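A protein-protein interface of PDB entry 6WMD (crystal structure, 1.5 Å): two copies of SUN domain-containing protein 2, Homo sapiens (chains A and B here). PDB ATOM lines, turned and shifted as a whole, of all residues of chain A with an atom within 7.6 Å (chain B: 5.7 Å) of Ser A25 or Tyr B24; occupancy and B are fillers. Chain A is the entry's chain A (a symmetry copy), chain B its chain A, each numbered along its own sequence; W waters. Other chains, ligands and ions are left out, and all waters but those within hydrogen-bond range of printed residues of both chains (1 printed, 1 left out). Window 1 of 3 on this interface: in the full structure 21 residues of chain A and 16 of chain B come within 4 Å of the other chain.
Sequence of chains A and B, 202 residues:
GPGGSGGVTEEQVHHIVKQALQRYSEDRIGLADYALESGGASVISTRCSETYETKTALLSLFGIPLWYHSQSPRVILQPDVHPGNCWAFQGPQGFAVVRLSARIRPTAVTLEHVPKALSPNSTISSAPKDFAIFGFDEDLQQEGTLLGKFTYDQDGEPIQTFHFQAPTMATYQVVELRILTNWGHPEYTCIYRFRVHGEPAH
Water W1 lies within hydrogen-bond range of the guanidinium group of Arg B28 (3.0 Å) and the side-chain hydroxyl of Ser A25 (3.5 Å).
Leu A21 touches Ala B20, but with the chains exchanged Ala A20 does not touch Leu B21 (7.8 Å).
Leu A21 touches its own counterpart, Leu B21.
Tyr A24 touches its own counterpart, Tyr B24.
Ser A25 touches Arg B28, but with the chains exchanged Arg A28 does not touch Ser B25 (12.8 Å).
Positions printed for both chains: 19, 20, 21, 22, 23, 24, 25, 26, 27, 28 and 29.
The side-chain carboxylate (OE1) of Glu A26 is in hydrogen-bond range of the side-chain amide nitrogen (NE2) of Gln A22, 2.9 Å away.
The guanidinium group (NE) of Arg A23 lies within salt-bridge range of the side-chain carboxylate (OE2) of Glu A26 (3.7 Å).
The side-chain hydroxyl of Ser A25 lies within hydrogen-bond range of the backbone carbonyl oxygen of Gln A22 (2.7 Å).
Of chain B, only Tyr B24 and Arg B28 come within 4 Å of Ser A25.
Tyr B24 touches just these residues of chain A: Leu A21, Tyr A24 and Ser A25.
Of the printed residues of chain A, Arg B28 touches Ser A25.
Of the printed residues of chain B, Glu A26 touches Leu B118 (3.6 Å).
Printed residues of chain B within 4 Å of Tyr A24: Tyr B24.
Of the printed residues of chain A, Ala B20 touches Leu A21.
Printed residues of chain A within 4 Å of Leu B21: Leu A21.
Lys A18 touches none of the printed residues of chain B.
The nearest residue of chain B that does not touch Ser A25 is Leu B118 (4.9 Å).
Of the 13 printed residues of chain A, 5 touch a printed residue of chain B.
Of the 13 printed residues of chain B, 5 touch a printed residue of chain A.
Along chain B the printed residues that touch a printed residue of chain A span positions 20 to 118.
Among the printed residues, 8 pairs touch across the chains.
Among the printed residues, merely in contact across the chains: Ser A25 with Tyr B24, Tyr A24 with Tyr B24, Ser A25 with Arg B28, Leu A21 with Leu B21, Glu A26 with Leu B118, Leu A21 with Tyr B24, Asp A27 with Leu B118 and Leu A21 with Ala B20.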
ATOM      1  N   LYS A  18     -17.669 -16.917  -3.880  1.00  0.00           N
ATOM      2  CA  LYS A  18     -18.154 -17.459  -5.143  1.00  0.00           C
ATOM      3  C   LYS A  18     -17.016 -18.061  -5.950  1.00  0.00           C
ATOM      4  O   LYS A  18     -17.129 -19.176  -6.470  1.00  0.00           O
ATOM      5  CB  LYS A  18     -18.854 -16.364  -5.955  1.00  0.00           C
ATOM      6  CG  LYS A  18     -19.480 -16.873  -7.253  1.00  0.00           C
ATOM      7  CD  LYS A  18     -20.128 -15.740  -8.033  1.00  0.00           C
ATOM      8  CE  LYS A  18     -20.153 -16.036  -9.525  1.00  0.00           C
ATOM      9  NZ  LYS A  18     -20.499 -14.819 -10.316  1.00  0.00           N
ATOM     10  N   GLN A  19     -15.898 -17.344  -6.050  1.00  0.00           N
ATOM     11  CA  GLN A  19     -14.788 -17.828  -6.865  1.00  0.00           C
ATOM     12  C   GLN A  19     -14.094 -19.029  -6.235  1.00  0.00           C
ATOM     13  O   GLN A  19     -13.635 -19.929  -6.955  1.00  0.00           O
ATOM     14  CB  GLN A  19     -13.831 -16.676  -7.133  1.00  0.00           C
ATOM     15  CG  GLN A  19     -14.510 -15.595  -7.954  1.00  0.00           C
ATOM     16  CD  GLN A  19     -13.528 -14.711  -8.666  1.00  0.00           C
ATOM     17  OE1 GLN A  19     -12.462 -14.410  -8.137  1.00  0.00           O
ATOM     18  NE2 GLN A  19     -13.884 -14.279  -9.873  1.00  0.00           N
ATOM     19  N   ALA A  20     -14.022 -19.083  -4.906  1.00  0.00           N
ATOM     20  CA  ALA A  20     -13.439 -20.252  -4.260  1.00  0.00           C
ATOM     21  C   ALA A  20     -14.299 -21.491  -4.482  1.00  0.00           C
ATOM     22  O   ALA A  20     -13.771 -22.588  -4.697  1.00  0.00           O
ATOM     23  CB  ALA A  20     -13.286 -19.984  -2.767  1.00  0.00           C
ATOM     24  N   LEU A  21     -15.622 -21.338  -4.426  1.00  0.00           N
ATOM     25  CA  LEU A  21     -16.502 -22.475  -4.678  1.00  0.00           C
ATOM     26  C   LEU A  21     -16.498 -22.874  -6.149  1.00  0.00           C
ATOM     27  O   LEU A  21     -16.641 -24.069  -6.463  1.00  0.00           O
ATOM     28  CB  LEU A  21     -17.914 -22.180  -4.173  1.00  0.00           C
ATOM     29  CG  LEU A  21     -18.086 -22.339  -2.664  1.00  0.00           C
ATOM     30  CD1 LEU A  21     -19.490 -21.914  -2.229  1.00  0.00           C
ATOM     31  CD2 LEU A  21     -17.822 -23.755  -2.237  1.00  0.00           C
ATOM     32  N   GLN A  22     -16.372 -21.905  -7.064  1.00  0.00           N
ATOM     33  CA  GLN A  22     -16.199 -22.247  -8.475  1.00  0.00           C
ATOM     34  C   GLN A  22     -14.993 -23.152  -8.652  1.00  0.00           C
ATOM     35  O   GLN A  22     -15.083 -24.234  -9.253  1.00  0.00           O
ATOM     36  CB  GLN A  22     -16.030 -20.984  -9.330  1.00  0.00           C
ATOM     37  CG  GLN A  22     -15.828 -21.291 -10.830  1.00  0.00           C
ATOM     38  CD  GLN A  22     -15.158 -20.171 -11.630  1.00  0.00           C
ATOM     39  OE1 GLN A  22     -15.209 -18.999 -11.256  1.00  0.00           O
ATOM     40  NE2 GLN A  22     -14.531 -20.540 -12.747  1.00  0.00           N
ATOM     41  N   ARG A  23     -13.849 -22.727  -8.120  1.00  0.00           N
ATOM     42  CA  ARG A  23     -12.640 -23.526  -8.271  1.00  0.00           C
ATOM     43  C   ARG A  23     -12.810 -24.900  -7.628  1.00  0.00           C
ATOM     44  O   ARG A  23     -12.410 -25.922  -8.206  1.00  0.00           O
ATOM     45  CB  ARG A  23     -11.448 -22.780  -7.673  1.00  0.00           C
ATOM     46  CG  ARG A  23     -10.191 -23.633  -7.551  1.00  0.00           C
ATOM     47  CD  ARG A  23      -9.634 -24.087  -8.901  1.00  0.00           C
ATOM     48  NE  ARG A  23      -9.762 -23.075  -9.947  1.00  0.00           N
ATOM     49  CZ  ARG A  23      -8.729 -22.491 -10.547  1.00  0.00           C
ATOM     50  NH1 ARG A  23      -8.931 -21.583 -11.492  1.00  0.00           N
ATOM     51  NH2 ARG A  23      -7.489 -22.808 -10.194  1.00  0.00           N
ATOM     52  N   TYR A  24     -13.422 -24.947  -6.441  1.00  0.00           N
ATOM     53  CA  TYR A  24     -13.672 -26.220  -5.773  1.00  0.00           C
ATOM     54  C   TYR A  24     -14.471 -27.153  -6.671  1.00  0.00           C
ATOM     55  O   TYR A  24     -14.136 -28.344  -6.803  1.00  0.00           O
ATOM     56  CB  TYR A  24     -14.419 -25.953  -4.454  1.00  0.00           C
ATOM     57  CG  TYR A  24     -14.488 -27.126  -3.507  1.00  0.00           C
ATOM     58  CD1 TYR A  24     -15.478 -28.084  -3.636  1.00  0.00           C
ATOM     59  CD2 TYR A  24     -13.557 -27.262  -2.474  1.00  0.00           C
ATOM     60  CE1 TYR A  24     -15.550 -29.171  -2.761  1.00  0.00           C
ATOM     61  CE2 TYR A  24     -13.625 -28.343  -1.597  1.00  0.00           C
ATOM     62  CZ  TYR A  24     -14.603 -29.288  -1.764  1.00  0.00           C
ATOM     63  OH  TYR A  24     -14.678 -30.367  -0.896  1.00  0.00           O
ATOM     64  N   SER A  25     -15.499 -26.615  -7.341  1.00  0.00           N
ATOM     65  CA  SER A  25     -16.370 -27.420  -8.187  1.00  0.00           C
ATOM     66  C   SER A  25     -15.682 -27.916  -9.447  1.00  0.00           C
ATOM     67  O   SER A  25     -16.154 -28.893 -10.038  1.00  0.00           O
ATOM     68  CB  SER A  25     -17.619 -26.620  -8.586  1.00  0.00           C
ATOM     69  OG  SER A  25     -17.327 -25.630  -9.558  1.00  0.00           O
ATOM     70  N   GLU A  26     -14.607 -27.262  -9.888  1.00  0.00           N
ATOM     71  CA  GLU A  26     -13.901 -27.659 -11.111  1.00  0.00           C
ATOM     72  C   GLU A  26     -12.841 -28.716 -10.796  1.00  0.00           C
ATOM     73  O   GLU A  26     -11.651 -28.533 -11.013  1.00  0.00           O
ATOM     74  CB  GLU A  26     -13.261 -26.442 -11.780  1.00  0.00           C
ATOM     75  CG  GLU A  26     -14.229 -25.397 -12.303  1.00  0.00           C
ATOM     76  CD  GLU A  26     -13.530 -24.127 -12.790  1.00  0.00           C
ATOM     77  OE1 GLU A  26     -14.203 -23.300 -13.452  1.00  0.00           O
ATOM     78  OE2 GLU A  26     -12.321 -23.939 -12.513  1.00  0.00           O
ATOM     79  N   ASP A  27     -13.299 -29.848 -10.255  1.00  0.00           N
ATOM     80  CA  ASP A  27     -12.393 -30.941  -9.904  1.00  0.00           C
ATOM     81  C   ASP A  27     -11.284 -30.429  -8.987  1.00  0.00           C
ATOM     82  O   ASP A  27     -10.137 -30.865  -9.072  1.00  0.00           O
ATOM     83  CB  ASP A  27     -11.825 -31.587 -11.180  1.00  0.00           C
ATOM     84  CG  ASP A  27     -11.382 -33.024 -11.011  1.00  0.00           C
ATOM     85  OD1 ASP A  27     -11.656 -33.669  -9.976  1.00  0.00           O
ATOM     86  OD2 ASP A  27     -10.758 -33.523 -11.985  1.00  0.00           O
ATOM     87  N   ARG A  28     -11.642 -29.472  -8.121  1.00  0.00           N
ATOM     88  CA  ARG A  28     -10.797 -28.849  -7.098  1.00  0.00           C
ATOM     89  C   ARG A  28      -9.696 -27.928  -7.607  1.00  0.00           C
ATOM     90  O   ARG A  28      -9.345 -26.969  -6.903  1.00  0.00           O
ATOM     91  CB  ARG A  28     -10.190 -29.871  -6.132  1.00  0.00           C
ATOM     92  CG  ARG A  28     -11.221 -30.659  -5.371  1.00  0.00           C
ATOM     93  CD  ARG A  28     -11.901 -29.819  -4.297  1.00  0.00           C
ATOM     94  NE  ARG A  28     -10.968 -29.055  -3.467  1.00  0.00           N
ATOM     95  CZ  ARG A  28     -10.381 -29.529  -2.374  1.00  0.00           C
ATOM     96  NH1 ARG A  28     -10.612 -30.774  -1.978  1.00  0.00           N
ATOM     97  NH2 ARG A  28      -9.553 -28.755  -1.677  1.00  0.00           N
ATOM     98  N   ILE A  29      -9.145 -28.206  -8.792  1.00  0.00           N
ATOM     99  CA  ILE A  29      -7.941 -27.529  -9.271  1.00  0.00           C
ATOM    100  C   ILE A  29      -8.121 -26.826 -10.606  1.00  0.00           C
ATOM    101  O   ILE A  29      -7.215 -26.085 -11.022  1.00  0.00           O
ATOM    102  CB  ILE A  29      -6.723 -28.474  -9.327  1.00  0.00           C
ATOM    103  CG1 ILE A  29      -6.908 -29.530 -10.420  1.00  0.00           C
ATOM    104  CG2 ILE A  29      -6.500 -29.131  -7.969  1.00  0.00           C
ATOM    105  CD1 ILE A  29      -5.716 -30.488 -10.530  1.00  0.00           C
ATOM    106  N   GLY A  30      -9.228 -27.041 -11.313  1.00  0.00           N
ATOM    107  CA  GLY A  30      -9.483 -26.253 -12.507  1.00  0.00           C
ATOM    108  C   GLY A  30      -8.606 -26.561 -13.700  1.00  0.00           C
ATOM    109  O   GLY A  30      -8.378 -25.672 -14.530  1.00  0.00           O
ATOM    110  N   GLN B  19     -23.401 -20.083   4.800  1.00  0.00           N
ATOM    111  CA  GLN B  19     -24.595 -20.178   3.967  1.00  0.00           C
ATOM    112  C   GLN B  19     -24.265 -20.561   2.530  1.00  0.00           C
ATOM    113  O   GLN B  19     -25.040 -21.284   1.887  1.00  0.00           O
ATOM    114  CB  GLN B  19     -25.370 -18.872   4.061  1.00  0.00           C
ATOM    115  CG  GLN B  19     -25.866 -18.642   5.476  1.00  0.00           C
ATOM    116  CD  GLN B  19     -27.021 -17.686   5.533  1.00  0.00           C
ATOM    117  OE1 GLN B  19     -27.073 -16.725   4.770  1.00  0.00           O
ATOM    118  NE2 GLN B  19     -27.955 -17.936   6.446  1.00  0.00           N
ATOM    119  N   ALA B  20     -23.122 -20.113   2.012  1.00  0.00           N
ATOM    120  CA  ALA B  20     -22.729 -20.521   0.668  1.00  0.00           C
ATOM    121  C   ALA B  20     -22.424 -22.014   0.613  1.00  0.00           C
ATOM    122  O   ALA B  20     -22.770 -22.687  -0.365  1.00  0.00           O
ATOM    123  CB  ALA B  20     -21.505 -19.723   0.233  1.00  0.00           C
ATOM    124  N   LEU B  21     -21.772 -22.548   1.646  1.00  0.00           N
ATOM    125  CA  LEU B  21     -21.494 -23.981   1.677  1.00  0.00           C
ATOM    126  C   LEU B  21     -22.760 -24.795   1.912  1.00  0.00           C
ATOM    127  O   LEU B  21     -22.875 -25.919   1.393  1.00  0.00           O
ATOM    128  CB  LEU B  21     -20.416 -24.293   2.715  1.00  0.00           C
ATOM    129  CG  LEU B  21     -18.993 -23.992   2.252  1.00  0.00           C
ATOM    130  CD1 LEU B  21     -17.991 -24.221   3.384  1.00  0.00           C
ATOM    131  CD2 LEU B  21     -18.624 -24.832   1.060  1.00  0.00           C
ATOM    132  N   GLN B  22     -23.704 -24.276   2.707  1.00  0.00           N
ATOM    133  CA  GLN B  22     -25.001 -24.939   2.834  1.00  0.00           C
ATOM    134  C   GLN B  22     -25.644 -25.101   1.469  1.00  0.00           C
ATOM    135  O   GLN B  22     -26.045 -26.207   1.075  1.00  0.00           O
ATOM    136  CB  GLN B  22     -25.936 -24.145   3.758  1.00  0.00           C
ATOM    137  CG  GLN B  22     -27.328 -24.796   3.913  1.00  0.00           C
ATOM    138  CD  GLN B  22     -28.435 -23.842   4.368  1.00  0.00           C
ATOM    139  OE1 GLN B  22     -28.177 -22.813   4.994  1.00  0.00           O
ATOM    140  NE2 GLN B  22     -29.681 -24.195   4.054  1.00  0.00           N
ATOM    141  N   ARG B  23     -25.741 -24.002   0.724  1.00  0.00           N
ATOM    142  CA  ARG B  23     -26.371 -24.071  -0.588  1.00  0.00           C
ATOM    143  C   ARG B  23     -25.615 -25.025  -1.508  1.00  0.00           C
ATOM    144  O   ARG B  23     -26.227 -25.826  -2.230  1.00  0.00           O
ATOM    145  CB  ARG B  23     -26.459 -22.670  -1.194  1.00  0.00           C
ATOM    146  CG  ARG B  23     -26.867 -22.664  -2.663  1.00  0.00           C
ATOM    147  CD  ARG B  23     -28.278 -23.200  -2.902  1.00  0.00           C
ATOM    148  NE  ARG B  23     -29.224 -22.821  -1.855  1.00  0.00           N
ATOM    149  CZ  ARG B  23     -30.279 -22.037  -2.053  1.00  0.00           C
ATOM    150  NH1 ARG B  23     -31.093 -21.745  -1.047  1.00  0.00           N
ATOM    151  NH2 ARG B  23     -30.518 -21.538  -3.259  1.00  0.00           N
ATOM    152  N   TYR B  24     -24.280 -24.968  -1.480  1.00  0.00           N
ATOM    153  CA  TYR B  24     -23.471 -25.875  -2.289  1.00  0.00           C
ATOM    154  C   TYR B  24     -23.817 -27.325  -1.983  1.00  0.00           C
ATOM    155  O   TYR B  24     -23.992 -28.141  -2.906  1.00  0.00           O
ATOM    156  CB  TYR B  24     -21.982 -25.594  -2.017  1.00  0.00           C
ATOM    157  CG  TYR B  24     -21.021 -26.235  -2.988  1.00  0.00           C
ATOM    158  CD1 TYR B  24     -20.596 -27.539  -2.808  1.00  0.00           C
ATOM    159  CD2 TYR B  24     -20.531 -25.517  -4.081  1.00  0.00           C
ATOM    160  CE1 TYR B  24     -19.704 -28.138  -3.701  1.00  0.00           C
ATOM    161  CE2 TYR B  24     -19.638 -26.108  -4.975  1.00  0.00           C
ATOM    162  CZ  TYR B  24     -19.255 -27.410  -4.784  1.00  0.00           C
ATOM    163  OH  TYR B  24     -18.367 -28.005  -5.667  1.00  0.00           O
ATOM    164  N   SER B  25     -23.973 -27.650  -0.693  1.00  0.00           N
ATOM    165  CA  SER B  25     -24.249 -29.018  -0.274  1.00  0.00           C
ATOM    166  C   SER B  25     -25.641 -29.490  -0.662  1.00  0.00           C
ATOM    167  O   SER B  25     -25.863 -30.704  -0.720  1.00  0.00           O
ATOM    168  CB  SER B  25     -24.085 -29.156   1.246  1.00  0.00           C
ATOM    169  OG  SER B  25     -25.158 -28.557   1.954  1.00  0.00           O
ATOM    170  N   GLU B  26     -26.582 -28.576  -0.901  1.00  0.00           N
ATOM    171  CA  GLU B  26     -27.956 -28.947  -1.255  1.00  0.00           C
ATOM    172  C   GLU B  26     -28.085 -29.137  -2.768  1.00  0.00           C
ATOM    173  O   GLU B  26     -28.844 -28.460  -3.450  1.00  0.00           O
ATOM    174  CB  GLU B  26     -28.940 -27.887  -0.763  1.00  0.00           C
ATOM    175  CG  GLU B  26     -29.037 -27.731   0.744  1.00  0.00           C
ATOM    176  CD  GLU B  26     -29.894 -26.537   1.167  1.00  0.00           C
ATOM    177  OE1 GLU B  26     -30.232 -26.451   2.372  1.00  0.00           O
ATOM    178  OE2 GLU B  26     -30.227 -25.679   0.313  1.00  0.00           O
ATOM    179  N   ASP B  27     -27.302 -30.081  -3.299  1.00  0.00           N
ATOM    180  CA  ASP B  27     -27.326 -30.364  -4.733  1.00  0.00           C
ATOM    181  C   ASP B  27     -27.074 -29.084  -5.526  1.00  0.00           C
ATOM    182  O   ASP B  27     -27.648 -28.874  -6.594  1.00  0.00           O
ATOM    183  CB  ASP B  27     -28.663 -31.021  -5.120  1.00  0.00           C
ATOM    184  CG  ASP B  27     -28.603 -31.875  -6.369  1.00  0.00           C
ATOM    185  OD1 ASP B  27     -27.512 -32.172  -6.898  1.00  0.00           O
ATOM    186  OD2 ASP B  27     -29.712 -32.283  -6.806  1.00  0.00           O
ATOM    187  N   ARG B  28     -26.222 -28.214  -4.968  1.00  0.00           N
ATOM    188  CA  ARG B  28     -25.762 -26.943  -5.535  1.00  0.00           C
ATOM    189  C   ARG B  28     -26.798 -25.828  -5.609  1.00  0.00           C
ATOM    190  O   ARG B  28     -26.417 -24.651  -5.512  1.00  0.00           O
ATOM    191  CB  ARG B  28     -25.109 -27.114  -6.911  1.00  0.00           C
ATOM    192  CG  ARG B  28     -23.896 -28.001  -6.891  1.00  0.00           C
ATOM    193  CD  ARG B  28     -22.701 -27.317  -6.238  1.00  0.00           C
ATOM    194  NE  ARG B  28     -22.465 -25.956  -6.722  1.00  0.00           N
ATOM    195  CZ  ARG B  28     -21.736 -25.660  -7.792  1.00  0.00           C
ATOM    196  NH1 ARG B  28     -21.178 -26.627  -8.509  1.00  0.00           N
ATOM    197  NH2 ARG B  28     -21.568 -24.390  -8.149  1.00  0.00           N
ATOM    198  N   ILE B  29     -28.077 -26.170  -5.791  1.00  0.00           N
ATOM    199  CA  ILE B  29     -29.112 -25.186  -6.097  1.00  0.00           C
ATOM    200  C   ILE B  29     -30.263 -25.177  -5.104  1.00  0.00           C
ATOM    201  O   ILE B  29     -31.110 -24.271  -5.176  1.00  0.00           O
ATOM    202  CB  ILE B  29     -29.650 -25.333  -7.536  1.00  0.00           C
ATOM    203  CG1 ILE B  29     -30.444 -26.634  -7.686  1.00  0.00           C
ATOM    204  CG2 ILE B  29     -28.504 -25.277  -8.539  1.00  0.00           C
ATOM    205  CD1 ILE B  29     -31.017 -26.824  -9.094  1.00  0.00           C
ATOM    206  N   PRO B 115     -17.520 -28.089 -17.099  1.00  0.00           N
ATOM    207  CA  PRO B 115     -16.956 -26.746 -17.279  1.00  0.00           C
ATOM    208  C   PRO B 115     -15.894 -26.697 -18.367  1.00  0.00           C
ATOM    209  O   PRO B 115     -15.159 -27.661 -18.603  1.00  0.00           O
ATOM    210  CB  PRO B 115     -16.309 -26.437 -15.923  1.00  0.00           C
ATOM    211  CG  PRO B 115     -16.637 -27.568 -15.015  1.00  0.00           C
ATOM    212  CD  PRO B 115     -17.178 -28.705 -15.807  1.00  0.00           C
ATOM    213  N   LEU B 118     -12.340 -27.811 -17.414  1.00  0.00           N
ATOM    214  CA  LEU B 118     -12.037 -29.239 -17.396  1.00  0.00           C
ATOM    215  C   LEU B 118     -12.070 -29.847 -18.791  1.00  0.00           C
ATOM    216  O   LEU B 118     -12.015 -31.077 -18.932  1.00  0.00           O
ATOM    217  CB  LEU B 118     -13.000 -29.976 -16.461  1.00  0.00           C
ATOM    218  CG  LEU B 118     -12.936 -29.470 -15.015  1.00  0.00           C
ATOM    219  CD1 LEU B 118     -13.869 -30.331 -14.163  1.00  0.00           C
ATOM    220  CD2 LEU B 118     -11.518 -29.526 -14.488  1.00  0.00           C
HETATM  221  O   HOH W   1     -20.289 -26.033 -11.305  1.00  0.00           O
